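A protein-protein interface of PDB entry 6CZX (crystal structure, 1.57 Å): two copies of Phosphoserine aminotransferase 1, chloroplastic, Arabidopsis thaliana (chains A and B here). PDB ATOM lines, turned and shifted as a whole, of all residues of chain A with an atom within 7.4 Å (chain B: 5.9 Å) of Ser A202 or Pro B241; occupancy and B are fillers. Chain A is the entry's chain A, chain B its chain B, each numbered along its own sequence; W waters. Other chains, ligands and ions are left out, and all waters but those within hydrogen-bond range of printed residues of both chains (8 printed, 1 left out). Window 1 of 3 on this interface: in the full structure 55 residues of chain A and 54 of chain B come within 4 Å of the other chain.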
ATOM      1  N   GLY A  11      -6.273 -11.297 -15.455  1.00  0.00           N
ATOM      2  CA  GLY A  11      -6.722 -12.644 -15.099  1.00  0.00           C
ATOM      3  C   GLY A  11      -7.872 -12.625 -14.105  1.00  0.00           C
ATOM      4  O   GLY A  11      -7.712 -12.047 -13.041  1.00  0.00           O
ATOM      5  N   PRO A  12      -9.033 -13.182 -14.447  1.00  0.00           N
ATOM      6  CA  PRO A  12      -9.370 -13.669 -15.791  1.00  0.00           C
ATOM      7  C   PRO A  12      -9.180 -12.557 -16.851  1.00  0.00           C
ATOM      8  O   PRO A  12      -8.950 -11.377 -16.505  1.00  0.00           O
ATOM      9  CB  PRO A  12     -10.855 -14.086 -15.661  1.00  0.00           C
ATOM     10  CG  PRO A  12     -10.998 -14.345 -14.188  1.00  0.00           C
ATOM     11  CD  PRO A  12     -10.196 -13.292 -13.540  1.00  0.00           C
ATOM     12  N   ALA A  13      -9.238 -12.946 -18.107  1.00  0.00           N
ATOM     13  CA  ALA A  13      -8.798 -12.072 -19.167  1.00  0.00           C
ATOM     14  C   ALA A  13      -9.606 -12.233 -20.431  1.00  0.00           C
ATOM     15  O   ALA A  13     -10.526 -13.080 -20.531  1.00  0.00           O
ATOM     16  CB  ALA A  13      -7.332 -12.332 -19.413  1.00  0.00           C
ATOM     17  N   LEU A  15     -10.824 -13.239 -24.103  1.00  0.00           N
ATOM     18  CA  LEU A  15     -10.851 -14.495 -24.875  1.00  0.00           C
ATOM     19  C   LEU A  15     -11.205 -14.217 -26.329  1.00  0.00           C
ATOM     20  O   LEU A  15     -11.799 -13.181 -26.622  1.00  0.00           O
ATOM     21  CB  LEU A  15     -11.915 -15.427 -24.304  1.00  0.00           C
ATOM     22  CG  LEU A  15     -11.563 -16.058 -22.975  1.00  0.00           C
ATOM     23  CD1 LEU A  15     -12.803 -16.668 -22.313  1.00  0.00           C
ATOM     24  CD2 LEU A  15     -10.386 -17.020 -23.139  1.00  0.00           C
ATOM     25  N   GLN A  74      -9.067 -28.645 -10.843  1.00  0.00           N
ATOM     26  CA  GLN A  74      -9.639 -27.453 -10.215  1.00  0.00           C
ATOM     27  C   GLN A  74      -8.677 -26.928  -9.170  1.00  0.00           C
ATOM     28  O   GLN A  74      -7.720 -27.627  -8.738  1.00  0.00           O
ATOM     29  CB  GLN A  74     -10.918 -27.832  -9.454  1.00  0.00           C
ATOM     30  CG  GLN A  74     -11.921 -28.607 -10.218  1.00  0.00           C
ATOM     31  CD  GLN A  74     -13.250 -28.792  -9.521  1.00  0.00           C
ATOM     32  OE1 GLN A  74     -13.875 -27.819  -8.983  1.00  0.00           O
ATOM     33  NE2 GLN A  74     -13.708 -30.052  -9.550  1.00  0.00           N
ATOM     34  N   GLY A 194      -2.846 -21.809 -14.111  1.00  0.00           N
ATOM     35  CA  GLY A 194      -4.282 -21.521 -14.239  1.00  0.00           C
ATOM     36  C   GLY A 194      -4.612 -21.210 -15.697  1.00  0.00           C
ATOM     37  O   GLY A 194      -3.824 -20.551 -16.385  1.00  0.00           O
ATOM     38  N   ALA A 195      -5.767 -21.671 -16.158  1.00  0.00           N
ATOM     39  CA  ALA A 195      -6.175 -21.414 -17.534  1.00  0.00           C
ATOM     40  C   ALA A 195      -6.580 -19.964 -17.787  1.00  0.00           C
ATOM     41  O   ALA A 195      -6.575 -19.513 -18.911  1.00  0.00           O
ATOM     42  CB  ALA A 195      -7.347 -22.300 -17.883  1.00  0.00           C
ATOM     43  N   GLN A 196      -6.953 -19.269 -16.731  1.00  0.00           N
ATOM     44  CA  GLN A 196      -7.755 -18.065 -16.892  1.00  0.00           C
ATOM     45  C   GLN A 196      -7.013 -16.919 -17.533  1.00  0.00           C
ATOM     46  O   GLN A 196      -7.660 -16.036 -18.082  1.00  0.00           O
ATOM     47  CB  GLN A 196      -8.393 -17.568 -15.599  1.00  0.00           C
ATOM     48  CG  GLN A 196      -7.436 -17.219 -14.492  1.00  0.00           C
ATOM     49  CD  GLN A 196      -7.046 -18.398 -13.593  1.00  0.00           C
ATOM     50  OE1 GLN A 196      -7.164 -19.579 -13.960  1.00  0.00           O
ATOM     51  NE2 GLN A 196      -6.557 -18.059 -12.399  1.00  0.00           N
ATOM     52  N1  LLP A 197       0.637 -17.626 -10.572  1.00  0.00           N
ATOM     53  C2  LLP A 197       0.603 -16.613 -11.459  1.00  0.00           C
ATOM     54  C2' LLP A 197       1.784 -16.331 -12.345  1.00  0.00           C
ATOM     55  C3  LLP A 197      -0.610 -15.834 -11.593  1.00  0.00           C
ATOM     56  O3  LLP A 197      -0.694 -14.791 -12.439  1.00  0.00           O
ATOM     57  C4  LLP A 197      -1.740 -16.163 -10.728  1.00  0.00           C
ATOM     58  C4' LLP A 197      -3.011 -15.374 -10.899  1.00  0.00           C
ATOM     59  C5  LLP A 197      -1.584 -17.308  -9.819  1.00  0.00           C
ATOM     60  C6  LLP A 197      -0.388 -17.982  -9.803  1.00  0.00           C
ATOM     61  C5' LLP A 197      -2.728 -17.701  -8.895  1.00  0.00           C
ATOM     62  OP4 LLP A 197      -3.669 -18.444  -9.700  1.00  0.00           O
ATOM     63  P   LLP A 197      -5.120 -18.827  -9.066  1.00  0.00           P
ATOM     64  OP1 LLP A 197      -5.707 -19.682 -10.124  1.00  0.00           O
ATOM     65  OP2 LLP A 197      -4.829 -19.622  -7.813  1.00  0.00           O
ATOM     66  OP3 LLP A 197      -5.770 -17.507  -8.833  1.00  0.00           O
ATOM     67  N   LLP A 197      -5.686 -16.931 -17.531  1.00  0.00           N
ATOM     68  CA  LLP A 197      -4.945 -15.816 -18.052  1.00  0.00           C
ATOM     69  CB  LLP A 197      -3.522 -15.765 -17.458  1.00  0.00           C
ATOM     70  CG  LLP A 197      -3.459 -15.248 -16.022  1.00  0.00           C
ATOM     71  CD  LLP A 197      -3.630 -16.234 -14.865  1.00  0.00           C
ATOM     72  CE  LLP A 197      -2.938 -15.754 -13.561  1.00  0.00           C
ATOM     73  NZ  LLP A 197      -3.618 -15.698 -12.227  1.00  0.00           N
ATOM     74  C   LLP A 197      -4.907 -15.897 -19.539  1.00  0.00           C
ATOM     75  O   LLP A 197      -5.332 -14.956 -20.204  1.00  0.00           O
ATOM     76  N   GLY A 200      -8.336 -19.929 -21.330  1.00  0.00           N
ATOM     77  CA  GLY A 200      -9.728 -20.274 -20.996  1.00  0.00           C
ATOM     78  C   GLY A 200     -10.225 -19.435 -19.867  1.00  0.00           C
ATOM     79  O   GLY A 200      -9.628 -18.447 -19.509  1.00  0.00           O
ATOM     80  N   PRO A 201     -11.383 -19.798 -19.324  1.00  0.00           N
ATOM     81  CA  PRO A 201     -11.938 -19.140 -18.156  1.00  0.00           C
ATOM     82  C   PRO A 201     -11.371 -19.687 -16.871  1.00  0.00           C
ATOM     83  O   PRO A 201     -10.657 -20.688 -16.882  1.00  0.00           O
ATOM     84  CB  PRO A 201     -13.423 -19.498 -18.255  1.00  0.00           C
ATOM     85  CG  PRO A 201     -13.383 -20.909 -18.825  1.00  0.00           C
ATOM     86  CD  PRO A 201     -12.119 -21.006 -19.679  1.00  0.00           C
ATOM     87  N   SER A 202     -11.628 -18.997 -15.757  1.00  0.00           N
ATOM     88  CA  SER A 202     -11.197 -19.489 -14.464  1.00  0.00           C
ATOM     89  C   SER A 202     -11.947 -20.749 -14.075  1.00  0.00           C
ATOM     90  O   SER A 202     -13.088 -20.928 -14.466  1.00  0.00           O
ATOM     91  CB  SER A 202     -11.366 -18.418 -13.397  1.00  0.00           C
ATOM     92  OG  SER A 202     -12.720 -18.053 -13.260  1.00  0.00           O
ATOM     93  N   GLY A 203     -11.292 -21.582 -13.285  1.00  0.00           N
ATOM     94  CA  GLY A 203     -11.878 -22.835 -12.811  1.00  0.00           C
ATOM     95  C   GLY A 203     -11.148 -24.077 -13.272  1.00  0.00           C
ATOM     96  O   GLY A 203     -11.459 -25.178 -12.767  1.00  0.00           O
ATOM     97  N   VAL A 204     -10.195 -23.912 -14.199  1.00  0.00           N
ATOM     98  CA  VAL A 204      -9.389 -24.983 -14.742  1.00  0.00           C
ATOM     99  C   VAL A 204      -7.929 -24.621 -14.529  1.00  0.00           C
ATOM    100  O   VAL A 204      -7.534 -23.469 -14.798  1.00  0.00           O
ATOM    101  CB  VAL A 204      -9.591 -25.213 -16.268  1.00  0.00           C
ATOM    102  CG1 VAL A 204      -8.731 -26.349 -16.769  1.00  0.00           C
ATOM    103  CG2 VAL A 204     -11.048 -25.484 -16.539  1.00  0.00           C
ATOM    104  N   THR A 205      -7.168 -25.585 -14.037  1.00  0.00           N
ATOM    105  CA  THR A 205      -5.712 -25.474 -13.938  1.00  0.00           C
ATOM    106  C   THR A 205      -5.092 -26.659 -14.677  1.00  0.00           C
ATOM    107  O   THR A 205      -5.555 -27.788 -14.541  1.00  0.00           O
ATOM    108  CB  THR A 205      -5.284 -25.576 -12.440  1.00  0.00           C
ATOM    109  OG1 THR A 205      -5.877 -24.509 -11.704  1.00  0.00           O
ATOM    110  CG2 THR A 205      -3.791 -25.482 -12.276  1.00  0.00           C
ATOM    111  N   PRO A 241     -14.130 -29.843 -13.965  1.00  0.00           N
ATOM    112  CA  PRO A 241     -14.750 -28.583 -14.405  1.00  0.00           C
ATOM    113  C   PRO A 241     -15.089 -28.708 -15.920  1.00  0.00           C
ATOM    114  O   PRO A 241     -14.351 -28.200 -16.765  1.00  0.00           O
ATOM    115  CB  PRO A 241     -13.667 -27.538 -14.104  1.00  0.00           C
ATOM    116  CG  PRO A 241     -12.363 -28.293 -14.229  1.00  0.00           C
ATOM    117  CD  PRO A 241     -12.668 -29.707 -13.786  1.00  0.00           C
ATOM    118  N   GLY A 244     -15.398 -25.511 -18.260  1.00  0.00           N
ATOM    119  CA  GLY A 244     -14.100 -24.899 -18.359  1.00  0.00           C
ATOM    120  C   GLY A 244     -13.180 -25.662 -19.273  1.00  0.00           C
ATOM    121  O   GLY A 244     -12.447 -25.059 -20.050  1.00  0.00           O
ATOM    122  N   MET B  38     -17.029 -14.761 -18.460  1.00  0.00           N
ATOM    123  CA  MET B  38     -15.792 -15.546 -18.533  1.00  0.00           C
ATOM    124  C   MET B  38     -14.514 -14.722 -18.674  1.00  0.00           C
ATOM    125  O   MET B  38     -13.423 -15.271 -18.503  1.00  0.00           O
ATOM    126  CB  MET B  38     -15.885 -16.555 -19.680  1.00  0.00           C
ATOM    127  CG  MET B  38     -16.702 -17.742 -19.288  1.00  0.00           C
ATOM    128  SD  MET B  38     -16.713 -19.016 -20.547  1.00  0.00           S
ATOM    129  CE  MET B  38     -18.045 -18.509 -21.581  1.00  0.00           C
ATOM    130  N   PHE B  47     -18.317  -8.407 -11.565  1.00  0.00           N
ATOM    131  CA  PHE B  47     -18.281  -9.714 -10.888  1.00  0.00           C
ATOM    132  C   PHE B  47     -18.667  -9.636  -9.424  1.00  0.00           C
ATOM    133  O   PHE B  47     -19.400 -10.492  -8.913  1.00  0.00           O
ATOM    134  CB  PHE B  47     -17.005 -10.523 -11.074  1.00  0.00           C
ATOM    135  CG  PHE B  47     -17.144 -11.890 -10.475  1.00  0.00           C
ATOM    136  CD1 PHE B  47     -17.955 -12.842 -11.101  1.00  0.00           C
ATOM    137  CD2 PHE B  47     -16.593 -12.194  -9.225  1.00  0.00           C
ATOM    138  CE1 PHE B  47     -18.173 -14.080 -10.500  1.00  0.00           C
ATOM    139  CE2 PHE B  47     -16.783 -13.444  -8.640  1.00  0.00           C
ATOM    140  CZ  PHE B  47     -17.594 -14.373  -9.279  1.00  0.00           C
ATOM    141  N   PHE B  72     -18.148 -19.926  -1.783  1.00  0.00           N
ATOM    142  CA  PHE B  72     -18.225 -20.469  -3.148  1.00  0.00           C
ATOM    143  C   PHE B  72     -16.808 -20.908  -3.507  1.00  0.00           C
ATOM    144  O   PHE B  72     -15.917 -20.059  -3.723  1.00  0.00           O
ATOM    145  CB  PHE B  72     -18.727 -19.441  -4.190  1.00  0.00           C
ATOM    146  CG  PHE B  72     -20.129 -19.028  -3.978  1.00  0.00           C
ATOM    147  CD1 PHE B  72     -21.162 -19.845  -4.357  1.00  0.00           C
ATOM    148  CD2 PHE B  72     -20.429 -17.800  -3.420  1.00  0.00           C
ATOM    149  CE1 PHE B  72     -22.499 -19.479  -4.144  1.00  0.00           C
ATOM    150  CE2 PHE B  72     -21.759 -17.422  -3.227  1.00  0.00           C
ATOM    151  CZ  PHE B  72     -22.787 -18.245  -3.604  1.00  0.00           C
ATOM    152  N   LEU B  73     -16.589 -22.211  -3.588  1.00  0.00           N
ATOM    153  CA  LEU B  73     -15.224 -22.758  -3.712  1.00  0.00           C
ATOM    154  C   LEU B  73     -15.084 -23.682  -4.920  1.00  0.00           C
ATOM    155  O   LEU B  73     -16.051 -24.048  -5.528  1.00  0.00           O
ATOM    156  CB  LEU B  73     -14.891 -23.570  -2.455  1.00  0.00           C
ATOM    157  CG  LEU B  73     -15.047 -22.837  -1.112  1.00  0.00           C
ATOM    158  CD1 LEU B  73     -14.666 -23.707   0.055  1.00  0.00           C
ATOM    159  CD2 LEU B  73     -14.225 -21.563  -1.125  1.00  0.00           C
ATOM    160  N   GLN B  74     -13.846 -24.031  -5.266  1.00  0.00           N
ATOM    161  CA  GLN B  74     -13.553 -25.075  -6.220  1.00  0.00           C
ATOM    162  C   GLN B  74     -13.182 -26.365  -5.515  1.00  0.00           C
ATOM    163  O   GLN B  74     -12.928 -26.381  -4.333  1.00  0.00           O
ATOM    164  CB  GLN B  74     -12.318 -24.660  -7.054  1.00  0.00           C
ATOM    165  CG  GLN B  74     -12.411 -23.302  -7.658  1.00  0.00           C
ATOM    166  CD  GLN B  74     -11.194 -22.992  -8.523  1.00  0.00           C
ATOM    167  OE1 GLN B  74     -10.866 -23.779  -9.450  1.00  0.00           O
ATOM    168  NE2 GLN B  74     -10.587 -21.805  -8.296  1.00  0.00           N
ATOM    169  N   GLY B 203     -17.755 -27.468 -11.027  1.00  0.00           N
ATOM    170  CA  GLY B 203     -16.622 -26.545 -10.856  1.00  0.00           C
ATOM    171  C   GLY B 203     -16.847 -25.594  -9.694  1.00  0.00           C
ATOM    172  O   GLY B 203     -15.928 -24.877  -9.319  1.00  0.00           O
ATOM    173  N   VAL B 204     -18.048 -25.575  -9.126  1.00  0.00           N
ATOM    174  CA  VAL B 204     -18.335 -24.829  -7.889  1.00  0.00           C
ATOM    175  C   VAL B 204     -18.823 -25.788  -6.806  1.00  0.00           C
ATOM    176  O   VAL B 204     -19.649 -26.668  -7.072  1.00  0.00           O
ATOM    177  CB  VAL B 204     -19.449 -23.779  -8.122  1.00  0.00           C
ATOM    178  CG1 VAL B 204     -19.812 -23.031  -6.851  1.00  0.00           C
ATOM    179  CG2 VAL B 204     -19.025 -22.838  -9.207  1.00  0.00           C
ATOM    180  N   THR B 239      -8.407 -16.742  -7.650  1.00  0.00           N
ATOM    181  CA  THR B 239      -9.377 -16.543  -8.741  1.00  0.00           C
ATOM    182  C   THR B 239     -10.482 -17.553  -8.615  1.00  0.00           C
ATOM    183  O   THR B 239     -10.229 -18.769  -8.647  1.00  0.00           O
ATOM    184  CB  THR B 239      -8.710 -16.637 -10.112  1.00  0.00           C
ATOM    185  OG1 THR B 239      -7.449 -15.934 -10.144  1.00  0.00           O
ATOM    186  CG2 THR B 239      -9.614 -16.047 -11.123  1.00  0.00           C
ATOM    187  N   PRO B 240     -11.729 -17.098  -8.372  1.00  0.00           N
ATOM    188  CA  PRO B 240     -12.797 -18.053  -8.143  1.00  0.00           C
ATOM    189  C   PRO B 240     -13.288 -18.609  -9.452  1.00  0.00           C
ATOM    190  O   PRO B 240     -12.896 -18.096 -10.493  1.00  0.00           O
ATOM    191  CB  PRO B 240     -13.877 -17.202  -7.496  1.00  0.00           C
ATOM    192  CG  PRO B 240     -13.670 -15.848  -8.017  1.00  0.00           C
ATOM    193  CD  PRO B 240     -12.195 -15.708  -8.305  1.00  0.00           C
ATOM    194  N   PRO B 241     -14.209 -19.589  -9.395  1.00  0.00           N
ATOM    195  CA  PRO B 241     -14.847 -20.124 -10.631  1.00  0.00           C
ATOM    196  C   PRO B 241     -15.962 -19.146 -11.080  1.00  0.00           C
ATOM    197  O   PRO B 241     -17.158 -19.397 -10.795  1.00  0.00           O
ATOM    198  CB  PRO B 241     -15.404 -21.488 -10.187  1.00  0.00           C
ATOM    199  CG  PRO B 241     -15.593 -21.321  -8.707  1.00  0.00           C
ATOM    200  CD  PRO B 241     -14.486 -20.418  -8.229  1.00  0.00           C
ATOM    201  N   CYS B 242     -15.571 -18.024 -11.706  1.00  0.00           N
ATOM    202  CA  CYS B 242     -16.506 -16.905 -11.916  1.00  0.00           C
ATOM    203  C   CYS B 242     -17.750 -17.340 -12.706  1.00  0.00           C
ATOM    204  O   CYS B 242     -18.902 -17.022 -12.324  1.00  0.00           O
ATOM    205  CB  CYS B 242     -15.846 -15.753 -12.639  1.00  0.00           C
ATOM    206  SG  CYS B 242     -14.508 -14.937 -11.721  1.00  0.00           S
ATOM    207  N   PHE B 243     -17.552 -18.047 -13.814  1.00  0.00           N
ATOM    208  CA  PHE B 243     -18.682 -18.393 -14.678  1.00  0.00           C
ATOM    209  C   PHE B 243     -19.601 -19.384 -13.953  1.00  0.00           C
ATOM    210  O   PHE B 243     -20.842 -19.283 -14.002  1.00  0.00           O
ATOM    211  CB  PHE B 243     -18.245 -18.974 -16.024  1.00  0.00           C
ATOM    212  CG  PHE B 243     -19.375 -19.103 -17.003  1.00  0.00           C
ATOM    213  CD1 PHE B 243     -19.932 -17.960 -17.579  1.00  0.00           C
ATOM    214  CD2 PHE B 243     -19.898 -20.345 -17.341  1.00  0.00           C
ATOM    215  CE1 PHE B 243     -21.002 -18.053 -18.470  1.00  0.00           C
ATOM    216  CE2 PHE B 243     -20.993 -20.448 -18.216  1.00  0.00           C
ATOM    217  CZ  PHE B 243     -21.518 -19.312 -18.792  1.00  0.00           C
ATOM    218  N   GLY B 244     -19.011 -20.317 -13.211  1.00  0.00           N
ATOM    219  CA  GLY B 244     -19.840 -21.242 -12.431  1.00  0.00           C
ATOM    220  C   GLY B 244     -20.674 -20.555 -11.375  1.00  0.00           C
ATOM    221  O   GLY B 244     -21.842 -20.919 -11.170  1.00  0.00           O
ATOM    222  N   ILE B 245     -20.083 -19.576 -10.677  1.00  0.00           N
ATOM    223  CA  ILE B 245     -20.807 -18.818  -9.656  1.00  0.00           C
ATOM    224  C   ILE B 245     -21.976 -18.042 -10.295  1.00  0.00           C
ATOM    225  O   ILE B 245     -23.118 -18.015  -9.796  1.00  0.00           O
ATOM    226  CB  ILE B 245     -19.847 -17.924  -8.855  1.00  0.00           C
ATOM    227  CG1 ILE B 245     -18.923 -18.810  -7.977  1.00  0.00           C
ATOM    228  CG2 ILE B 245     -20.610 -16.869  -8.041  1.00  0.00           C
ATOM    229  CD1 ILE B 245     -17.699 -18.120  -7.422  1.00  0.00           C
ATOM    230  N   TYR B 246     -21.701 -17.436 -11.431  1.00  0.00           N
ATOM    231  CA  TYR B 246     -22.715 -16.736 -12.224  1.00  0.00           C
ATOM    232  C   TYR B 246     -23.868 -17.667 -12.558  1.00  0.00           C
ATOM    233  O   TYR B 246     -25.025 -17.338 -12.346  1.00  0.00           O
ATOM    234  CB  TYR B 246     -22.034 -16.175 -13.462  1.00  0.00           C
ATOM    235  CG  TYR B 246     -22.970 -15.905 -14.595  1.00  0.00           C
ATOM    236  CD1 TYR B 246     -23.826 -14.770 -14.617  1.00  0.00           C
ATOM    237  CD2 TYR B 246     -23.033 -16.783 -15.655  1.00  0.00           C
ATOM    238  CE1 TYR B 246     -24.690 -14.562 -15.700  1.00  0.00           C
ATOM    239  CE2 TYR B 246     -23.904 -16.576 -16.713  1.00  0.00           C
ATOM    240  CZ  TYR B 246     -24.702 -15.453 -16.732  1.00  0.00           C
ATOM    241  OH  TYR B 246     -25.556 -15.273 -17.786  1.00  0.00           O
HETATM  242  O   HOH W   1     -13.316 -16.612 -16.058  1.00  0.00           O
HETATM  243  O   HOH W   2     -16.226 -27.532  -7.385  1.00  0.00           O
HETATM  244  O   HOH W   3     -14.999 -18.554 -15.059  1.00  0.00           O
HETATM  245  O   HOH W   4      -8.642 -23.983 -11.420  1.00  0.00           O
HETATM  246  O   HOH W   5     -13.772 -24.893 -11.119  1.00  0.00           O
HETATM  247  O   HOH W   6     -16.146 -21.173 -13.525  1.00  0.00           O
HETATM  248  O   HOH W   7      -8.324 -20.350  -9.794  1.00  0.00           O
HETATM  249  O   HOH W   8      -6.064 -14.747 -12.296  1.00  0.00           O
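Water W8 lies within hydrogen-bond range of NZ of LLP A197, OG1 of Thr B239, O of Gly A11 and NE2 of Gln A196.
Water W7 lies within hydrogen-bond range of OP1 of LLP A197 (2.7 Å), O of Thr B239 (2.7 Å) and NE2 of Gln B74 (3.1 Å).
Water W1 bridges O of Met B38 (2.8 Å) and N of Ser A202 (2.9 Å).
Water W5 bridges O of Gly B203 (2.8 Å) and O of Gly A203 (2.9 Å).
Water W3 lies within hydrogen-bond range of the backbone NH of Phe B243 (2.9 Å), the side-chain hydroxyl of Ser A202 (2.9 Å) and the backbone NH of Cys B242 (3.4 Å).
Water W6 lies within hydrogen-bond range of the backbone NH (N) of Gly B244 (3.0 Å), the backbone carbonyl oxygen (O) of Ser A202 (3.2 Å), the backbone carbonyl oxygen (O) of Pro B241 (3.4 Å) and the backbone NH (N) of Phe B243 (3.4 Å).
Of the 15 printed residues of chain B, 7 touch a printed residue of chain A.
Printed residues of chain B that touch a printed residue of chain A: Met B38, Gln B74, Gly B203, Thr B239, Pro B240, Pro B241 and Cys B242.
Of the 17 printed residues of chain A, 7 touch a printed residue of chain B.
Printed residues of chain A that touch a printed residue of chain B: Pro A12, Gln A74, Gln A196, LLP A197, Pro A201, Ser A202 and Gly A203.
Hydrophobic or aromatic side chains of chain A within 4 Å of the printed part of chain B: Pro A12 and Pro A201.
Along chain A the printed residues that touch a printed residue of chain B span positions 12 to 203.
Among the printed residues, 11 pairs touch across the chains.
Among the printed residues, no Asp or Glu carboxylate lies within 4 Å of a Lys or Arg side-chain nitrogen of the other chain.
Gln B74 touches its own counterpart, Gln A74.
Gln A74 touches Gly B203, and with the chains exchanged Gly A203 touches Gln B74.
Positions printed for both chains: 74, 203, 204, 241 and 244.
Of the 11 pairs that touch across the chains among the printed residues, 3 have their exchanged pair printed and touching as well.
The backbone NH of Ala A13 lies within hydrogen-bond range of the backbone carbonyl oxygen of Gln A196 (3.5 Å).
The side-chain amide nitrogen (NE2) of Gln A196 sits at hydrogen-bond distance from OP1 of LLP A197 (2.9 Å).
NE2 of Gln B74 sits at hydrogen-bond distance from O of Thr B239, 3.1 Å away.
The side-chain sulfur of Cys B242 is in hydrogen-bond range of the backbone carbonyl oxygen of Pro B240 (3.8 Å).
NE2 of Gln A196 sits at hydrogen-bond distance from OG1 of Thr B239.
OP3 of LLP A197 sits at hydrogen-bond distance from OG1 of Thr B239 (2.6 Å).
The side-chain hydroxyl (OG) of Ser A202 sits at hydrogen-bond distance from the backbone carbonyl oxygen (O) of Pro B240, 2.8 Å away.
N of Cys B242 lies within hydrogen-bond range of OG of Ser A202 (3.2 Å).
Among the printed residues, pairs that only touch across the chains: Gln A74 with Gly B203 (3.6 Å), Gly A203 with Gln B74 (3.6 Å), Pro A12 with Thr B239 (3.7 Å), Ser A202 with Thr B239 (3.7 Å), Gln A74 with Gln B74 (3.8 Å), Pro A201 with Met B38 (3.9 Å) and Ser A202 with Pro B241 (3.97 Å).
Gly A200 touches none of the printed residues of chain B.
Printed residues of chain B within 4 Å of Ser A202: Thr B239, Pro B240, Pro B241 and Cys B242.
Printed residues of chain B within 4 Å of Gly A203: Gln B74 (3.6 Å).
Pro A241 touches none of the printed residues of chain B.
Printed residues of chain A within 4 Å of Pro B241: Ser A202 (3.97 Å).
Of the printed residues of chain A, Cys B242 touches Ser A202 (3.2 Å).
The nearest printed residue of chain A that does not touch Gln B74 is Val A204 (4.8 Å).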
